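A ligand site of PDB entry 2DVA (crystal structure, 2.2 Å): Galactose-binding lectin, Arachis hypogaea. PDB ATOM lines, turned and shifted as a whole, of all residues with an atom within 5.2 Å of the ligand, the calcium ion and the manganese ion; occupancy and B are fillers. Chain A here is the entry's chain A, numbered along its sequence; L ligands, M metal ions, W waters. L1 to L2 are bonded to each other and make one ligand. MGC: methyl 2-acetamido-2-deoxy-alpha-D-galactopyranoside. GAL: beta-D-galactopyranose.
The backbone NH (N) of Gly 104 lies within hydrogen-bond range of an oxygen (O3) of GAL L2 (2.9 Å).
ND2 of Asn 127 lies within hydrogen-bond range of O3 of GAL L2, at 2.8 Å.
O6 of GAL L2 sits at hydrogen-bond distance from OD2 of Asp 80.
The side-chain hydroxyl (OG) of Ser 211 is in hydrogen-bond range of an oxygen (O4) of GAL L2.
An oxygen (O4) of MGC L1 is in hydrogen-bond range of the backbone NH (N) of Gly 213.
N of Leu 212 sits at hydrogen-bond distance from O4 of MGC L1 (3.3 Å).
O3 of GAL L2 is in hydrogen-bond range of OD1 of Asp 83, at 2.6 Å.
The backbone carbonyl oxygen (O) of Gly 213 sits at hydrogen-bond distance from the backbone NH (N) of Asp 80, 3.0 Å away.
The side-chain hydroxyl (OG) of Ser 211 lies within hydrogen-bond range of the backbone NH (N) of Gly 214 (2.9 Å).
N of Gly 104 is in hydrogen-bond range of OD1 of Asp 83.
O of Gly 210 sits at hydrogen-bond distance from N of Gly 103 (2.9 Å).
The side-chain amide nitrogen of Asn 127 sits at hydrogen-bond distance from the side-chain carboxylate of Glu 129, at 3.1 Å.
CB of Ala 82 touches O4 of GAL L2 (3.6 Å).
Gly 103 touches the ligand.
Gly 214 touches the ligand.
Of the 23 residues printed, 11 come within 4 Å of the ligand.
The nearest printed residue that does not touch the ligand is Glu 129 (4.2 Å).
Within 4 Å of the calcium ion: Asp 123, Tyr 125, Asn 127 and Asp 132.
The calcium ion is bound by the backbone carbonyl oxygen (O) of Tyr 125 (2.5 Å).
OD1 of Asn 127 is bound to the calcium ion (2.5 Å).
The calcium ion is bound by OD2 of Asp 132 (2.6 Å).
The calcium ion is bound by water W13.
The calcium ion is bound by OD1 of Asp 123 (2.6 Å).
Water W2 binds the calcium ion, at 2.6 Å.
OD2 of Asp 123 is bound to the calcium ion (2.7 Å).
The manganese ion is bound by the side-chain carboxylate of Asp 123 (2.2 Å), the side-chain carboxylate of Glu 121 (2.2 Å), the side-chain carboxylate of Asp 132 (2.2 Å), water W11 (2.3 Å), water W9 (2.3 Å) and a ring nitrogen (NE2) of His 137 (2.4 Å).
The manganese ion has six donor atoms within binding distance.
Water W9 bridges O of Val 145 (2.6 Å) and OE1 of Glu 121 (2.6 Å).
Water W7 bridges O2 of GAL L2 (2.6 Å) and N of Gly 104 (3.1 Å).
Water W3 lies within hydrogen-bond range of the side-chain amide nitrogen of Asn 41 (2.6 Å), an oxygen (O7) of MGC L1 (2.8 Å) and the backbone NH of Leu 212 (3.1 Å).
Water W5 lies within hydrogen-bond range of OE2 of Glu 129 (2.8 Å), O2 of GAL L2 (2.9 Å) and ND2 of Asn 127 (3.5 Å).
Water W10 lies within hydrogen-bond range of OH of Tyr 125 and O6 of GAL L2.
Water W1 bridges the backbone carbonyl oxygen (O) of Ile 101 (2.7 Å) and an oxygen (O7) of MGC L1 (3.1 Å).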
ATOM      1  N   ASN A  41     -17.453  31.706  -7.008  1.00  0.00           N
ATOM      2  CA  ASN A  41     -17.395  31.500  -8.461  1.00  0.00           C
ATOM      3  C   ASN A  41     -16.421  30.415  -8.870  1.00  0.00           C
ATOM      4  O   ASN A  41     -15.635  30.587  -9.801  1.00  0.00           O
ATOM      5  CB  ASN A  41     -17.002  32.810  -9.170  1.00  0.00           C
ATOM      6  CG  ASN A  41     -18.042  33.895  -9.021  1.00  0.00           C
ATOM      7  OD1 ASN A  41     -17.842  35.028  -9.449  1.00  0.00           O
ATOM      8  ND2 ASN A  41     -19.175  33.554  -8.417  1.00  0.00           N
ATOM      9  N   ASP A  80     -26.916  27.330  -1.644  1.00  0.00           N
ATOM     10  CA  ASP A  80     -27.966  26.906  -2.544  1.00  0.00           C
ATOM     11  C   ASP A  80     -27.297  25.898  -3.497  1.00  0.00           C
ATOM     12  O   ASP A  80     -26.246  26.188  -4.060  1.00  0.00           O
ATOM     13  CB  ASP A  80     -28.495  28.130  -3.306  1.00  0.00           C
ATOM     14  CG  ASP A  80     -29.703  27.821  -4.160  1.00  0.00           C
ATOM     15  OD1 ASP A  80     -30.554  27.012  -3.739  1.00  0.00           O
ATOM     16  OD2 ASP A  80     -29.809  28.404  -5.250  1.00  0.00           O
ATOM     17  N   ALA A  82     -26.045  24.574  -6.390  1.00  0.00           N
ATOM     18  CA  ALA A  82     -25.825  25.045  -7.760  1.00  0.00           C
ATOM     19  C   ALA A  82     -24.354  24.804  -8.121  1.00  0.00           C
ATOM     20  O   ALA A  82     -23.544  24.585  -7.220  1.00  0.00           O
ATOM     21  CB  ALA A  82     -26.174  26.520  -7.858  1.00  0.00           C
ATOM     22  N   ASP A  83     -23.988  24.857  -9.399  1.00  0.00           N
ATOM     23  CA  ASP A  83     -24.903  25.145 -10.514  1.00  0.00           C
ATOM     24  C   ASP A  83     -25.199  23.953 -11.424  1.00  0.00           C
ATOM     25  O   ASP A  83     -26.190  23.965 -12.161  1.00  0.00           O
ATOM     26  CB  ASP A  83     -24.338  26.293 -11.353  1.00  0.00           C
ATOM     27  CG  ASP A  83     -24.695  27.645 -10.801  1.00  0.00           C
ATOM     28  OD1 ASP A  83     -25.770  28.161 -11.164  1.00  0.00           O
ATOM     29  OD2 ASP A  83     -23.916  28.177  -9.989  1.00  0.00           O
ATOM     30  N   ILE A 101     -17.218  33.987 -14.323  1.00  0.00           N
ATOM     31  CA  ILE A 101     -17.968  34.237 -13.108  1.00  0.00           C
ATOM     32  C   ILE A 101     -18.575  32.930 -12.607  1.00  0.00           C
ATOM     33  O   ILE A 101     -19.289  32.902 -11.607  1.00  0.00           O
ATOM     34  CB  ILE A 101     -19.111  35.255 -13.331  1.00  0.00           C
ATOM     35  CG1 ILE A 101     -20.134  34.684 -14.321  1.00  0.00           C
ATOM     36  CG2 ILE A 101     -18.548  36.585 -13.843  1.00  0.00           C
ATOM     37  CD1 ILE A 101     -21.360  35.573 -14.494  1.00  0.00           C
ATOM     38  N   GLY A 103     -20.918  30.136 -11.843  1.00  0.00           N
ATOM     39  CA  GLY A 103     -22.363  30.134 -11.745  1.00  0.00           C
ATOM     40  C   GLY A 103     -23.065  29.451 -12.913  1.00  0.00           C
ATOM     41  O   GLY A 103     -22.704  28.335 -13.319  1.00  0.00           O
ATOM     42  N   GLY A 104     -24.058  30.141 -13.467  1.00  0.00           N
ATOM     43  CA  GLY A 104     -24.824  29.598 -14.572  1.00  0.00           C
ATOM     44  C   GLY A 104     -24.068  29.372 -15.871  1.00  0.00           C
ATOM     45  O   GLY A 104     -24.599  28.733 -16.784  1.00  0.00           O
ATOM     46  N   GLU A 121     -25.859  19.429 -20.620  1.00  0.00           N
ATOM     47  CA  GLU A 121     -25.841  19.951 -19.262  1.00  0.00           C
ATOM     48  C   GLU A 121     -26.863  19.312 -18.342  1.00  0.00           C
ATOM     49  O   GLU A 121     -27.913  18.831 -18.783  1.00  0.00           O
ATOM     50  CB  GLU A 121     -26.031  21.474 -19.273  1.00  0.00           C
ATOM     51  CG  GLU A 121     -27.339  21.895 -19.918  1.00  0.00           C
ATOM     52  CD  GLU A 121     -27.714  23.322 -19.584  1.00  0.00           C
ATOM     53  OE1 GLU A 121     -26.993  24.249 -20.005  1.00  0.00           O
ATOM     54  OE2 GLU A 121     -28.733  23.503 -18.898  1.00  0.00           O
ATOM     55  N   ASP A 123     -28.348  20.823 -15.356  1.00  0.00           N
ATOM     56  CA  ASP A 123     -28.574  22.075 -14.672  1.00  0.00           C
ATOM     57  C   ASP A 123     -29.435  22.027 -13.422  1.00  0.00           C
ATOM     58  O   ASP A 123     -30.582  21.583 -13.487  1.00  0.00           O
ATOM     59  CB  ASP A 123     -29.214  23.026 -15.679  1.00  0.00           C
ATOM     60  CG  ASP A 123     -28.847  24.432 -15.429  1.00  0.00           C
ATOM     61  OD1 ASP A 123     -28.639  24.781 -14.248  1.00  0.00           O
ATOM     62  OD2 ASP A 123     -28.792  25.203 -16.407  1.00  0.00           O
ATOM     63  N   TYR A 125     -30.038  24.908 -11.320  1.00  0.00           N
ATOM     64  CA  TYR A 125     -30.443  26.239 -10.887  1.00  0.00           C
ATOM     65  C   TYR A 125     -31.020  26.990 -12.073  1.00  0.00           C
ATOM     66  O   TYR A 125     -30.457  26.964 -13.159  1.00  0.00           O
ATOM     67  CB  TYR A 125     -29.275  27.018 -10.285  1.00  0.00           C
ATOM     68  CG  TYR A 125     -29.660  28.424  -9.888  1.00  0.00           C
ATOM     69  CD1 TYR A 125     -29.594  29.467 -10.815  1.00  0.00           C
ATOM     70  CD2 TYR A 125     -30.163  28.703  -8.616  1.00  0.00           C
ATOM     71  CE1 TYR A 125     -30.036  30.743 -10.497  1.00  0.00           C
ATOM     72  CE2 TYR A 125     -30.616  29.987  -8.281  1.00  0.00           C
ATOM     73  CZ  TYR A 125     -30.552  31.006  -9.226  1.00  0.00           C
ATOM     74  OH  TYR A 125     -30.996  32.271  -8.927  1.00  0.00           O
ATOM     75  N   SER A 126     -32.139  27.674 -11.881  1.00  0.00           N
ATOM     76  CA  SER A 126     -32.763  28.396 -12.990  1.00  0.00           C
ATOM     77  C   SER A 126     -32.256  29.825 -13.228  1.00  0.00           C
ATOM     78  O   SER A 126     -32.716  30.766 -12.574  1.00  0.00           O
ATOM     79  CB  SER A 126     -34.273  28.431 -12.797  1.00  0.00           C
ATOM     80  OG  SER A 126     -34.920  28.915 -13.954  1.00  0.00           O
ATOM     81  N   ASN A 127     -31.316  29.976 -14.156  1.00  0.00           N
ATOM     82  CA  ASN A 127     -30.774  31.291 -14.506  1.00  0.00           C
ATOM     83  C   ASN A 127     -31.633  31.894 -15.608  1.00  0.00           C
ATOM     84  O   ASN A 127     -31.537  31.516 -16.775  1.00  0.00           O
ATOM     85  CB  ASN A 127     -29.336  31.199 -15.015  1.00  0.00           C
ATOM     86  CG  ASN A 127     -28.376  30.722 -13.950  1.00  0.00           C
ATOM     87  OD1 ASN A 127     -28.400  29.552 -13.585  1.00  0.00           O
ATOM     88  ND2 ASN A 127     -27.528  31.610 -13.446  1.00  0.00           N
ATOM     89  N   GLU A 129     -31.355  34.729 -16.918  1.00  0.00           N
ATOM     90  CA  GLU A 129     -30.525  35.423 -17.894  1.00  0.00           C
ATOM     91  C   GLU A 129     -30.076  34.485 -19.024  1.00  0.00           C
ATOM     92  O   GLU A 129     -29.565  34.937 -20.045  1.00  0.00           O
ATOM     93  CB  GLU A 129     -29.294  36.044 -17.228  1.00  0.00           C
ATOM     94  CG  GLU A 129     -28.284  35.045 -16.695  1.00  0.00           C
ATOM     95  CD  GLU A 129     -28.513  34.706 -15.240  1.00  0.00           C
ATOM     96  OE1 GLU A 129     -29.673  34.639 -14.809  1.00  0.00           O
ATOM     97  OE2 GLU A 129     -27.500  34.498 -14.536  1.00  0.00           O
ATOM     98  N   ASP A 132     -33.286  29.628 -18.695  1.00  0.00           N
ATOM     99  CA  ASP A 132     -33.477  28.290 -18.158  1.00  0.00           C
ATOM    100  C   ASP A 132     -34.931  27.964 -17.857  1.00  0.00           C
ATOM    101  O   ASP A 132     -35.720  28.851 -17.540  1.00  0.00           O
ATOM    102  CB  ASP A 132     -32.733  28.094 -16.842  1.00  0.00           C
ATOM    103  CG  ASP A 132     -31.275  27.842 -17.019  1.00  0.00           C
ATOM    104  OD1 ASP A 132     -30.891  27.171 -18.000  1.00  0.00           O
ATOM    105  OD2 ASP A 132     -30.503  28.314 -16.171  1.00  0.00           O
ATOM    106  N   PRO A 133     -35.296  26.679 -17.958  1.00  0.00           N
ATOM    107  CA  PRO A 133     -36.685  26.287 -17.656  1.00  0.00           C
ATOM    108  C   PRO A 133     -36.804  26.580 -16.165  1.00  0.00           C
ATOM    109  O   PRO A 133     -35.817  26.871 -15.507  1.00  0.00           O
ATOM    110  CB  PRO A 133     -36.694  24.784 -17.945  1.00  0.00           C
ATOM    111  CG  PRO A 133     -35.615  24.619 -18.960  1.00  0.00           C
ATOM    112  CD  PRO A 133     -34.530  25.534 -18.463  1.00  0.00           C
ATOM    113  N   HIS A 137     -32.985  20.482 -15.020  1.00  0.00           N
ATOM    114  CA  HIS A 137     -33.153  19.991 -16.370  1.00  0.00           C
ATOM    115  C   HIS A 137     -31.866  19.513 -17.037  1.00  0.00           C
ATOM    116  O   HIS A 137     -30.760  19.820 -16.594  1.00  0.00           O
ATOM    117  CB  HIS A 137     -33.744  21.102 -17.233  1.00  0.00           C
ATOM    118  CG  HIS A 137     -32.947  22.373 -17.187  1.00  0.00           C
ATOM    119  ND1 HIS A 137     -32.978  23.244 -16.119  1.00  0.00           N
ATOM    120  CD2 HIS A 137     -32.050  22.892 -18.067  1.00  0.00           C
ATOM    121  CE1 HIS A 137     -32.143  24.238 -16.340  1.00  0.00           C
ATOM    122  NE2 HIS A 137     -31.569  24.051 -17.506  1.00  0.00           N
ATOM    123  N   VAL A 145     -25.063  28.510 -23.130  1.00  0.00           N
ATOM    124  CA  VAL A 145     -25.739  27.865 -22.005  1.00  0.00           C
ATOM    125  C   VAL A 145     -27.235  28.119 -22.093  1.00  0.00           C
ATOM    126  O   VAL A 145     -28.002  27.664 -21.247  1.00  0.00           O
ATOM    127  CB  VAL A 145     -25.204  28.327 -20.628  1.00  0.00           C
ATOM    128  CG1 VAL A 145     -23.808  27.762 -20.399  1.00  0.00           C
ATOM    129  CG2 VAL A 145     -25.195  29.838 -20.535  1.00  0.00           C
ATOM    130  N   SER A 147     -29.701  26.799 -23.663  1.00  0.00           N
ATOM    131  CA  SER A 147     -29.950  25.548 -24.361  1.00  0.00           C
ATOM    132  C   SER A 147     -30.806  25.562 -25.626  1.00  0.00           C
ATOM    133  O   SER A 147     -31.858  26.215 -25.693  1.00  0.00           O
ATOM    134  CB  SER A 147     -30.537  24.526 -23.367  1.00  0.00           C
ATOM    135  OG  SER A 147     -29.608  24.243 -22.332  1.00  0.00           O
ATOM    136  N   GLY A 210     -19.851  27.159  -9.554  1.00  0.00           N
ATOM    137  CA  GLY A 210     -20.721  27.642  -8.495  1.00  0.00           C
ATOM    138  C   GLY A 210     -20.570  29.155  -8.425  1.00  0.00           C
ATOM    139  O   GLY A 210     -19.810  29.742  -9.196  1.00  0.00           O
ATOM    140  N   SER A 211     -21.312  29.799  -7.524  1.00  0.00           N
ATOM    141  CA  SER A 211     -21.227  31.246  -7.377  1.00  0.00           C
ATOM    142  C   SER A 211     -20.907  31.557  -5.922  1.00  0.00           C
ATOM    143  O   SER A 211     -20.397  30.699  -5.199  1.00  0.00           O
ATOM    144  CB  SER A 211     -22.556  31.893  -7.777  1.00  0.00           C
ATOM    145  OG  SER A 211     -23.634  31.434  -6.973  1.00  0.00           O
ATOM    146  N   LEU A 212     -21.185  32.784  -5.482  1.00  0.00           N
ATOM    147  CA  LEU A 212     -20.901  33.140  -4.091  1.00  0.00           C
ATOM    148  C   LEU A 212     -21.840  32.357  -3.177  1.00  0.00           C
ATOM    149  O   LEU A 212     -21.408  31.758  -2.194  1.00  0.00           O
ATOM    150  CB  LEU A 212     -21.070  34.649  -3.859  1.00  0.00           C
ATOM    151  CG  LEU A 212     -20.652  35.166  -2.471  1.00  0.00           C
ATOM    152  CD1 LEU A 212     -20.288  36.641  -2.548  1.00  0.00           C
ATOM    153  CD2 LEU A 212     -21.763  34.946  -1.477  1.00  0.00           C
ATOM    154  N   GLY A 213     -23.120  32.356  -3.529  1.00  0.00           N
ATOM    155  CA  GLY A 213     -24.107  31.655  -2.718  1.00  0.00           C
ATOM    156  C   GLY A 213     -24.515  30.293  -3.239  1.00  0.00           C
ATOM    157  O   GLY A 213     -25.074  29.491  -2.483  1.00  0.00           O
ATOM    158  N   GLY A 214     -24.237  30.016  -4.505  1.00  0.00           N
ATOM    159  CA  GLY A 214     -24.607  28.729  -5.079  1.00  0.00           C
ATOM    160  C   GLY A 214     -23.425  27.782  -5.144  1.00  0.00           C
ATOM    161  O   GLY A 214     -22.517  27.967  -5.959  1.00  0.00           O
HETATM  162  O6  MGC L   1     -25.446  36.531  -2.234  1.00  0.00           O
HETATM  163  C6  MGC L   1     -25.482  35.423  -3.111  1.00  0.00           C
HETATM  164  C5  MGC L   1     -25.594  35.846  -4.574  1.00  0.00           C
HETATM  165  O5  MGC L   1     -24.494  36.838  -4.966  1.00  0.00           O
HETATM  166  C1  MGC L   1     -24.543  37.413  -6.352  1.00  0.00           C
HETATM  167  O1  MGC L   1     -25.796  38.129  -6.509  1.00  0.00           O
HETATM  168  CM  MGC L   1     -26.019  39.535  -5.854  1.00  0.00           C
HETATM  169  C2  MGC L   1     -24.420  36.245  -7.345  1.00  0.00           C
HETATM  170  N2  MGC L   1     -24.486  36.892  -8.610  1.00  0.00           N
HETATM  171  C7  MGC L   1     -23.754  36.549  -9.714  1.00  0.00           C
HETATM  172  O7  MGC L   1     -22.649  35.970  -9.665  1.00  0.00           O
HETATM  173  C8  MGC L   1     -24.335  36.911 -11.068  1.00  0.00           C
HETATM  174  C3  MGC L   1     -25.528  35.200  -7.070  1.00  0.00           C
HETATM  175  O3  MGC L   1     -25.290  34.152  -7.941  1.00  0.00           O
HETATM  176  C4  MGC L   1     -25.516  34.612  -5.598  1.00  0.00           C
HETATM  177  O4  MGC L   1     -24.286  33.850  -5.450  1.00  0.00           O
HETATM  178  C1  GAL L   2     -26.193  33.275  -8.581  1.00  0.00           C
HETATM  179  C2  GAL L   2     -25.691  32.610  -9.847  1.00  0.00           C
HETATM  180  C3  GAL L   2     -26.505  31.352 -10.196  1.00  0.00           C
HETATM  181  C4  GAL L   2     -26.556  30.296  -8.956  1.00  0.00           C
HETATM  182  C5  GAL L   2     -27.206  31.034  -7.750  1.00  0.00           C
HETATM  183  C6  GAL L   2     -27.583  30.535  -6.377  1.00  0.00           C
HETATM  184  O2  GAL L   2     -25.767  33.616 -10.849  1.00  0.00           O
HETATM  185  O3  GAL L   2     -25.895  30.709 -11.319  1.00  0.00           O
HETATM  186  O4  GAL L   2     -25.242  29.918  -8.520  1.00  0.00           O
HETATM  187  O5  GAL L   2     -26.356  32.265  -7.462  1.00  0.00           O
HETATM  188  O6  GAL L   2     -28.460  30.948  -5.352  1.00  0.00           O
HETATM  189 CA    CA M   1     -28.566  27.312 -14.792  1.00  0.00          CA
HETATM  190 MN    MN M   2     -29.747  25.337 -18.333  1.00  0.00          MN
HETATM  191  O   HOH W   1     -21.921  33.457 -11.263  1.00  0.00           O
HETATM  192  O   HOH W   2     -26.875  27.683 -16.797  1.00  0.00           O
HETATM  193  O   HOH W   3     -21.159  35.042  -7.533  1.00  0.00           O
HETATM  194  O   HOH W   4     -25.461  40.763  -9.079  1.00  0.00           O
HETATM  195  O   HOH W   5     -28.252  34.650 -11.871  1.00  0.00           O
HETATM  196  O   HOH W   6     -25.067  37.374 -14.367  1.00  0.00           O
HETATM  197  O   HOH W   7     -24.042  33.183 -12.790  1.00  0.00           O
HETATM  198  O   HOH W   8     -27.480  37.886  -8.948  1.00  0.00           O
HETATM  199  O   HOH W   9     -27.821  26.478 -18.936  1.00  0.00           O
HETATM  200  O   HOH W  10     -30.189  33.074  -6.509  1.00  0.00           O
HETATM  201  O   HOH W  11     -30.922  25.345 -20.319  1.00  0.00           O
HETATM  202  O   HOH W  12     -27.487  32.158  -3.249  1.00  0.00           O
HETATM  203  O   HOH W  13     -26.799  26.474 -13.107  1.00  0.00           O
HETATM  204  O   HOH W  14     -27.382  37.789 -12.246  1.00  0.00           O
